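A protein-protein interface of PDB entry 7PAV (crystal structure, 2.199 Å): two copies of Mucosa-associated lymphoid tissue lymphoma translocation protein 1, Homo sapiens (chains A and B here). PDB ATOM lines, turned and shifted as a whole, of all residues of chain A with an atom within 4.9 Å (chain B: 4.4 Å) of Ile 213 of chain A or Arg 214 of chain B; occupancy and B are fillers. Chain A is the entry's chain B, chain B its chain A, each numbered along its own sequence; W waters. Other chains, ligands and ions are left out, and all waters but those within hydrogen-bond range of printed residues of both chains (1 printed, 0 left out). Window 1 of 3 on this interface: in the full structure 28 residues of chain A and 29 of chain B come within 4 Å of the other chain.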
ATOM      1  N   VAL A 150      -9.509 -35.454  18.448  1.00  0.00           N
ATOM      2  CA  VAL A 150      -8.985 -34.991  17.164  1.00  0.00           C
ATOM      3  C   VAL A 150     -10.047 -35.193  16.043  1.00  0.00           C
ATOM      4  O   VAL A 150     -10.571 -36.276  15.851  1.00  0.00           O
ATOM      5  CB  VAL A 150      -7.613 -35.636  16.802  1.00  0.00           C
ATOM      6  CG1 VAL A 150      -7.030 -35.033  15.523  1.00  0.00           C
ATOM      7  CG2 VAL A 150      -6.620 -35.513  17.974  1.00  0.00           C
ATOM      8  N   PHE A 151     -10.391 -34.114  15.359  1.00  0.00           N
ATOM      9  CA  PHE A 151     -11.308 -34.081  14.239  1.00  0.00           C
ATOM     10  C   PHE A 151     -10.518 -33.805  12.996  1.00  0.00           C
ATOM     11  O   PHE A 151      -9.767 -32.840  12.948  1.00  0.00           O
ATOM     12  CB  PHE A 151     -12.296 -32.925  14.386  1.00  0.00           C
ATOM     13  CG  PHE A 151     -13.558 -33.287  15.109  1.00  0.00           C
ATOM     14  CD1 PHE A 151     -13.604 -33.294  16.489  1.00  0.00           C
ATOM     15  CD2 PHE A 151     -14.704 -33.610  14.408  1.00  0.00           C
ATOM     16  CE1 PHE A 151     -14.771 -33.648  17.156  1.00  0.00           C
ATOM     17  CE2 PHE A 151     -15.881 -33.911  15.075  1.00  0.00           C
ATOM     18  CZ  PHE A 151     -15.903 -33.966  16.442  1.00  0.00           C
ATOM     19  N   GLY A 152     -10.720 -34.623  11.987  1.00  0.00           N
ATOM     20  CA  GLY A 152     -10.131 -34.442  10.675  1.00  0.00           C
ATOM     21  C   GLY A 152     -11.282 -34.351   9.696  1.00  0.00           C
ATOM     22  O   GLY A 152     -11.956 -35.353   9.438  1.00  0.00           O
ATOM     23  N   THR A 189      -2.281 -35.797  15.212  1.00  0.00           N
ATOM     24  CA  THR A 189      -2.438 -34.394  14.792  1.00  0.00           C
ATOM     25  C   THR A 189      -1.351 -33.995  13.797  1.00  0.00           C
ATOM     26  O   THR A 189      -1.623 -33.294  12.834  1.00  0.00           O
ATOM     27  CB  THR A 189      -2.398 -33.468  16.001  1.00  0.00           C
ATOM     28  OG1 THR A 189      -1.211 -33.733  16.742  1.00  0.00           O
ATOM     29  CG2 THR A 189      -3.600 -33.632  16.878  1.00  0.00           C
ATOM     30  N   LEU A 192      -2.216 -35.932  10.499  1.00  0.00           N
ATOM     31  CA  LEU A 192      -3.277 -35.224   9.773  1.00  0.00           C
ATOM     32  C   LEU A 192      -2.787 -33.921   9.143  1.00  0.00           C
ATOM     33  O   LEU A 192      -3.198 -33.587   8.033  1.00  0.00           O
ATOM     34  CB  LEU A 192      -4.498 -34.960  10.680  1.00  0.00           C
ATOM     35  CG  LEU A 192      -5.322 -36.212  11.026  1.00  0.00           C
ATOM     36  CD1 LEU A 192      -6.519 -35.873  11.906  1.00  0.00           C
ATOM     37  CD2 LEU A 192      -5.782 -36.943   9.769  1.00  0.00           C
ATOM     38  N   ASP A 193      -1.897 -33.187   9.840  1.00  0.00           N
ATOM     39  CA  ASP A 193      -1.332 -31.937   9.337  1.00  0.00           C
ATOM     40  C   ASP A 193      -0.444 -32.188   8.102  1.00  0.00           C
ATOM     41  O   ASP A 193      -0.422 -31.379   7.170  1.00  0.00           O
ATOM     42  CB  ASP A 193      -0.567 -31.256  10.463  1.00  0.00           C
ATOM     43  CG  ASP A 193       0.189 -30.015  10.086  1.00  0.00           C
ATOM     44  OD1 ASP A 193      -0.417 -28.912  10.128  1.00  0.00           O
ATOM     45  OD2 ASP A 193       1.408 -30.133   9.788  1.00  0.00           O
ATOM     46  N   ALA A 196      -2.659 -32.791   5.125  1.00  0.00           N
ATOM     47  CA  ALA A 196      -3.147 -31.487   4.651  1.00  0.00           C
ATOM     48  C   ALA A 196      -2.122 -30.822   3.727  1.00  0.00           C
ATOM     49  O   ALA A 196      -2.500 -30.226   2.725  1.00  0.00           O
ATOM     50  CB  ALA A 196      -3.467 -30.569   5.827  1.00  0.00           C
ATOM     51  N   LEU A 211      -8.167 -29.941   3.928  1.00  0.00           N
ATOM     52  CA  LEU A 211      -8.596 -30.641   5.125  1.00  0.00           C
ATOM     53  C   LEU A 211      -8.413 -29.736   6.354  1.00  0.00           C
ATOM     54  O   LEU A 211      -7.529 -28.867   6.402  1.00  0.00           O
ATOM     55  CB  LEU A 211      -7.998 -32.066   5.238  1.00  0.00           C
ATOM     56  CG  LEU A 211      -6.928 -32.404   6.237  1.00  0.00           C
ATOM     57  CD1 LEU A 211      -7.528 -32.861   7.560  1.00  0.00           C
ATOM     58  CD2 LEU A 211      -6.139 -33.544   5.710  1.00  0.00           C
ATOM     59  N   GLU A 212      -9.395 -29.797   7.252  1.00  0.00           N
ATOM     60  CA  GLU A 212      -9.373 -28.974   8.462  1.00  0.00           C
ATOM     61  C   GLU A 212      -9.253 -29.853   9.679  1.00  0.00           C
ATOM     62  O   GLU A 212      -9.931 -30.865   9.792  1.00  0.00           O
ATOM     63  CB  GLU A 212     -10.599 -28.078   8.557  1.00  0.00           C
ATOM     64  CG  GLU A 212     -10.463 -27.027   9.646  1.00  0.00           C
ATOM     65  CD  GLU A 212     -11.756 -26.374  10.076  1.00  0.00           C
ATOM     66  OE1 GLU A 212     -12.403 -25.692   9.246  1.00  0.00           O
ATOM     67  OE2 GLU A 212     -12.116 -26.536  11.262  1.00  0.00           O
ATOM     68  N   ILE A 213      -8.345 -29.499  10.568  1.00  0.00           N
ATOM     69  CA  ILE A 213      -8.089 -30.264  11.771  1.00  0.00           C
ATOM     70  C   ILE A 213      -8.493 -29.478  12.969  1.00  0.00           C
ATOM     71  O   ILE A 213      -8.096 -28.346  13.077  1.00  0.00           O
ATOM     72  CB  ILE A 213      -6.583 -30.625  11.839  1.00  0.00           C
ATOM     73  CG1 ILE A 213      -6.135 -31.365  10.592  1.00  0.00           C
ATOM     74  CG2 ILE A 213      -6.278 -31.477  13.066  1.00  0.00           C
ATOM     75  CD1 ILE A 213      -4.796 -31.104  10.275  1.00  0.00           C
ATOM     76  N   ARG A 214      -9.317 -30.035  13.858  1.00  0.00           N
ATOM     77  CA  ARG A 214      -9.671 -29.371  15.139  1.00  0.00           C
ATOM     78  C   ARG A 214      -9.225 -30.346  16.203  1.00  0.00           C
ATOM     79  O   ARG A 214      -9.658 -31.508  16.201  1.00  0.00           O
ATOM     80  CB  ARG A 214     -11.161 -29.081  15.289  1.00  0.00           C
ATOM     81  CG  ARG A 214     -11.702 -28.216  14.188  1.00  0.00           C
ATOM     82  CD  ARG A 214     -13.082 -27.720  14.551  1.00  0.00           C
ATOM     83  NE  ARG A 214     -13.737 -26.999  13.453  1.00  0.00           N
ATOM     84  CZ  ARG A 214     -15.032 -26.684  13.435  1.00  0.00           C
ATOM     85  NH1 ARG A 214     -15.825 -27.042  14.440  1.00  0.00           N
ATOM     86  NH2 ARG A 214     -15.545 -26.024  12.409  1.00  0.00           N
ATOM     87  N   SER A 215      -8.275 -29.930  17.022  1.00  0.00           N
ATOM     88  CA  SER A 215      -7.718 -30.816  18.016  1.00  0.00           C
ATOM     89  C   SER A 215      -7.498 -30.207  19.372  1.00  0.00           C
ATOM     90  O   SER A 215      -6.982 -29.104  19.509  1.00  0.00           O
ATOM     91  CB  SER A 215      -6.419 -31.423  17.496  1.00  0.00           C
ATOM     92  OG  SER A 215      -5.558 -31.856  18.541  1.00  0.00           O
ATOM     93  N   ARG B 128     -14.509 -19.298  26.201  1.00  0.00           N
ATOM     94  CA  ARG B 128     -15.280 -19.752  25.053  1.00  0.00           C
ATOM     95  C   ARG B 128     -16.669 -20.199  25.419  1.00  0.00           C
ATOM     96  O   ARG B 128     -17.169 -21.138  24.836  1.00  0.00           O
ATOM     97  CB  ARG B 128     -14.499 -20.842  24.318  1.00  0.00           C
ATOM     98  CG  ARG B 128     -13.246 -20.312  23.683  1.00  0.00           C
ATOM     99  CD  ARG B 128     -12.478 -21.390  22.979  1.00  0.00           C
ATOM    100  NE  ARG B 128     -13.218 -21.938  21.835  1.00  0.00           N
ATOM    101  CZ  ARG B 128     -12.882 -23.053  21.195  1.00  0.00           C
ATOM    102  NH1 ARG B 128     -11.835 -23.766  21.592  1.00  0.00           N
ATOM    103  NH2 ARG B 128     -13.618 -23.493  20.182  1.00  0.00           N
ATOM    104  N   ILE B 149      -5.296 -20.882   7.375  1.00  0.00           N
ATOM    105  CA  ILE B 149      -5.873 -20.370   8.589  1.00  0.00           C
ATOM    106  C   ILE B 149      -5.490 -21.224   9.789  1.00  0.00           C
ATOM    107  O   ILE B 149      -5.654 -22.444   9.770  1.00  0.00           O
ATOM    108  CB  ILE B 149      -7.408 -20.290   8.442  1.00  0.00           C
ATOM    109  CG1 ILE B 149      -7.806 -19.461   7.225  1.00  0.00           C
ATOM    110  CG2 ILE B 149      -8.027 -19.728   9.736  1.00  0.00           C
ATOM    111  CD1 ILE B 149      -9.218 -19.634   6.833  1.00  0.00           C
ATOM    112  N   VAL B 150      -4.956 -20.587  10.821  1.00  0.00           N
ATOM    113  CA  VAL B 150      -4.648 -21.271  12.062  1.00  0.00           C
ATOM    114  C   VAL B 150      -5.258 -20.546  13.254  1.00  0.00           C
ATOM    115  O   VAL B 150      -4.956 -19.379  13.473  1.00  0.00           O
ATOM    116  CB  VAL B 150      -3.140 -21.513  12.280  1.00  0.00           C
ATOM    117  CG1 VAL B 150      -2.917 -22.216  13.616  1.00  0.00           C
ATOM    118  CG2 VAL B 150      -2.543 -22.335  11.144  1.00  0.00           C
ATOM    119  N   PHE B 151      -6.106 -21.226  14.028  1.00  0.00           N
ATOM    120  CA  PHE B 151      -6.625 -20.671  15.284  1.00  0.00           C
ATOM    121  C   PHE B 151      -5.917 -21.368  16.422  1.00  0.00           C
ATOM    122  O   PHE B 151      -5.736 -22.596  16.401  1.00  0.00           O
ATOM    123  CB  PHE B 151      -8.128 -20.917  15.469  1.00  0.00           C
ATOM    124  CG  PHE B 151      -9.017 -19.977  14.707  1.00  0.00           C
ATOM    125  CD1 PHE B 151      -9.235 -20.149  13.354  1.00  0.00           C
ATOM    126  CD2 PHE B 151      -9.630 -18.916  15.339  1.00  0.00           C
ATOM    127  CE1 PHE B 151     -10.057 -19.275  12.647  1.00  0.00           C
ATOM    128  CE2 PHE B 151     -10.430 -18.034  14.625  1.00  0.00           C
ATOM    129  CZ  PHE B 151     -10.649 -18.226  13.284  1.00  0.00           C
ATOM    130  N   TYR B 153      -6.686 -21.439  20.296  1.00  0.00           N
ATOM    131  CA  TYR B 153      -7.555 -21.049  21.402  1.00  0.00           C
ATOM    132  C   TYR B 153      -6.903 -21.370  22.740  1.00  0.00           C
ATOM    133  O   TYR B 153      -6.369 -22.460  22.909  1.00  0.00           O
ATOM    134  CB  TYR B 153      -8.926 -21.731  21.344  1.00  0.00           C
ATOM    135  CG  TYR B 153      -9.693 -21.529  20.055  1.00  0.00           C
ATOM    136  CD1 TYR B 153      -9.569 -22.427  19.003  1.00  0.00           C
ATOM    137  CD2 TYR B 153     -10.648 -20.528  19.941  1.00  0.00           C
ATOM    138  CE1 TYR B 153     -10.312 -22.279  17.841  1.00  0.00           C
ATOM    139  CE2 TYR B 153     -11.388 -20.363  18.782  1.00  0.00           C
ATOM    140  CZ  TYR B 153     -11.210 -21.234  17.728  1.00  0.00           C
ATOM    141  OH  TYR B 153     -11.958 -21.095  16.589  1.00  0.00           O
ATOM    142  N   GLN B 157     -13.903 -25.358  23.788  1.00  0.00           N
ATOM    143  CA  GLN B 157     -15.226 -24.775  23.588  1.00  0.00           C
ATOM    144  C   GLN B 157     -16.120 -25.033  24.782  1.00  0.00           C
ATOM    145  O   GLN B 157     -16.183 -26.159  25.252  1.00  0.00           O
ATOM    146  CB  GLN B 157     -15.836 -25.376  22.321  1.00  0.00           C
ATOM    147  CG  GLN B 157     -17.119 -24.715  21.855  1.00  0.00           C
ATOM    148  CD  GLN B 157     -17.497 -25.223  20.483  1.00  0.00           C
ATOM    149  OE1 GLN B 157     -16.633 -25.494  19.628  1.00  0.00           O
ATOM    150  NE2 GLN B 157     -18.798 -25.349  20.241  1.00  0.00           N
ATOM    151  N   GLU B 212      -6.883 -25.513  22.279  1.00  0.00           N
ATOM    152  CA  GLU B 212      -7.548 -26.071  21.119  1.00  0.00           C
ATOM    153  C   GLU B 212      -6.951 -25.449  19.859  1.00  0.00           C
ATOM    154  O   GLU B 212      -6.759 -24.239  19.798  1.00  0.00           O
ATOM    155  CB  GLU B 212      -9.077 -25.959  21.144  1.00  0.00           C
ATOM    156  CG  GLU B 212      -9.662 -26.835  20.046  1.00  0.00           C
ATOM    157  CD  GLU B 212     -11.094 -26.617  19.600  1.00  0.00           C
ATOM    158  OE1 GLU B 212     -11.362 -26.830  18.395  1.00  0.00           O
ATOM    159  OE2 GLU B 212     -11.953 -26.280  20.447  1.00  0.00           O
ATOM    160  N   ILE B 213      -6.602 -26.289  18.883  1.00  0.00           N
ATOM    161  CA  ILE B 213      -6.015 -25.871  17.616  1.00  0.00           C
ATOM    162  C   ILE B 213      -6.946 -26.242  16.502  1.00  0.00           C
ATOM    163  O   ILE B 213      -7.361 -27.377  16.385  1.00  0.00           O
ATOM    164  CB  ILE B 213      -4.605 -26.474  17.419  1.00  0.00           C
ATOM    165  CG1 ILE B 213      -3.613 -25.775  18.323  1.00  0.00           C
ATOM    166  CG2 ILE B 213      -4.139 -26.372  15.972  1.00  0.00           C
ATOM    167  CD1 ILE B 213      -3.125 -26.656  19.339  1.00  0.00           C
ATOM    168  N   ARG B 214      -7.319 -25.275  15.726  1.00  0.00           N
ATOM    169  CA  ARG B 214      -8.222 -25.445  14.603  1.00  0.00           C
ATOM    170  C   ARG B 214      -7.368 -24.962  13.437  1.00  0.00           C
ATOM    171  O   ARG B 214      -6.764 -23.905  13.540  1.00  0.00           O
ATOM    172  CB  ARG B 214      -9.416 -24.537  14.852  1.00  0.00           C
ATOM    173  CG  ARG B 214     -10.618 -24.711  13.982  1.00  0.00           C
ATOM    174  CD  ARG B 214     -11.777 -24.018  14.684  1.00  0.00           C
ATOM    175  NE  ARG B 214     -12.238 -24.790  15.848  1.00  0.00           N
ATOM    176  CZ  ARG B 214     -13.406 -24.598  16.461  1.00  0.00           C
ATOM    177  NH1 ARG B 214     -14.227 -23.636  16.055  1.00  0.00           N
ATOM    178  NH2 ARG B 214     -13.765 -25.378  17.477  1.00  0.00           N
ATOM    179  N   SER B 215      -7.218 -25.760  12.381  1.00  0.00           N
ATOM    180  CA  SER B 215      -6.299 -25.392  11.299  1.00  0.00           C
ATOM    181  C   SER B 215      -6.596 -25.981   9.971  1.00  0.00           C
ATOM    182  O   SER B 215      -6.832 -27.167   9.860  1.00  0.00           O
ATOM    183  CB  SER B 215      -4.868 -25.758  11.703  1.00  0.00           C
ATOM    184  OG  SER B 215      -3.941 -25.709  10.632  1.00  0.00           O
HETATM  185  O   HOH W   1      -3.200 -28.105   9.236  1.00  0.00           O
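O of Arg 214 of chain A lies within hydrogen-bond range of N of Phe 151 of chain A, 2.8 Å away. NH1 of Arg 128 of chain B is in salt-bridge range of OE2 of Glu 212 of chain B (2.8 Å). The side-chain carboxylate of Glu 212 of chain A lies within salt-bridge range of the guanidinium group of Arg 214 of chain A (2.8 Å). The backbone NH (N) of Phe 151 of chain B lies within hydrogen-bond range of the backbone carbonyl oxygen (O) of Arg 214 of chain B (2.8 Å). The side-chain carboxylate (OE1) of Glu 212 of chain B is in salt-bridge range of the guanidinium group (NH2) of Arg 214 of chain B. OH of Tyr 153 of chain B lies within hydrogen-bond range of NH1 of Arg 214 of chain B (3.4 Å).
Water W1 lies within hydrogen-bond range of OG of Ser 215 of chain B (2.9 Å) and OD1 of Asp 193 of chain A (3.0 Å).
Of chain B, only Ile 213 (3.5 Å), Arg 214 (3.3 Å) and Ser 215 (2.8 Å) come within 4 Å of Ile 213 of chain A. Of the printed residues of chain A, Ser 215 of chain B touches Leu 211 (3.9 Å), Glu 212 (3.4 Å) and Ile 213 (2.8 Å). Printed residues of chain A within 4 Å of Ile 213 of chain B: Ile 213, Arg 214 and Ser 215. Of the printed residues of chain B, Ser 215 of chain A touches Glu 212 (3.5 Å) and Ile 213 (2.8 Å). Of the printed residues of chain B, Leu 211 of chain A touches Ser 215 (3.9 Å). Phe 151 of chain A touches none of the printed residues of chain B. The nearest printed residue of chain A that does not touch Glu 212 of chain B is Ile 213 of chain A (6.4 Å).
O of Ile 213 of chain B sits at hydrogen-bond distance from N of Ser 215 of chain A (2.8 Å). The backbone carbonyl oxygen (O) of Ile 213 of chain A is in hydrogen-bond range of the backbone NH (N) of Ser 215 of chain B.
Printed residues of chain B that touch a printed residue of chain A: Glu 212, Ile 213, Arg 214 and Ser 215. Among the printed residues, 11 pairs touch across the chains. Among the printed residues, no Asp or Glu carboxylate lies within 4 Å of a Lys or Arg side-chain nitrogen of the other chain.
Ile 213 of chain B touches its own counterpart, Ile 213 of chain A. Ile 213 of chain A touches Arg 214 of chain B, and with the chains exchanged Arg 214 of chain A touches Ile 213 of chain B. Ile 213 of chain A touches Ser 215 of chain B, and with the chains exchanged Ser 215 of chain A touches Ile 213 of chain B. Arg 214 of chain B touches its own counterpart, Arg 214 of chain A.
Ser 215 of chain B touches Leu 211 of chain A. OE2 of Glu 212 of chain A touches CG of Arg 214 of chain B (3.6 Å). O of Ser 215 of chain B touches CA of Glu 212 of chain A, at 3.4 Å. Ile 213 of chain A touches Ile 213 of chain B. CA of Arg 214 of chain B touches O of Ile 213 of chain A, at 3.3 Å. CB of Arg 214 of chain A touches OE1 of Glu 212 of chain B (3.8 Å). Arg 214 of chain A touches Ile 213 of chain B. Arg 214 of chain B touches Arg 214 of chain A (NE to CD, 3.3 Å). Ser 215 of chain A touches Glu 212 of chain B (O to CA, 3.5 Å).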
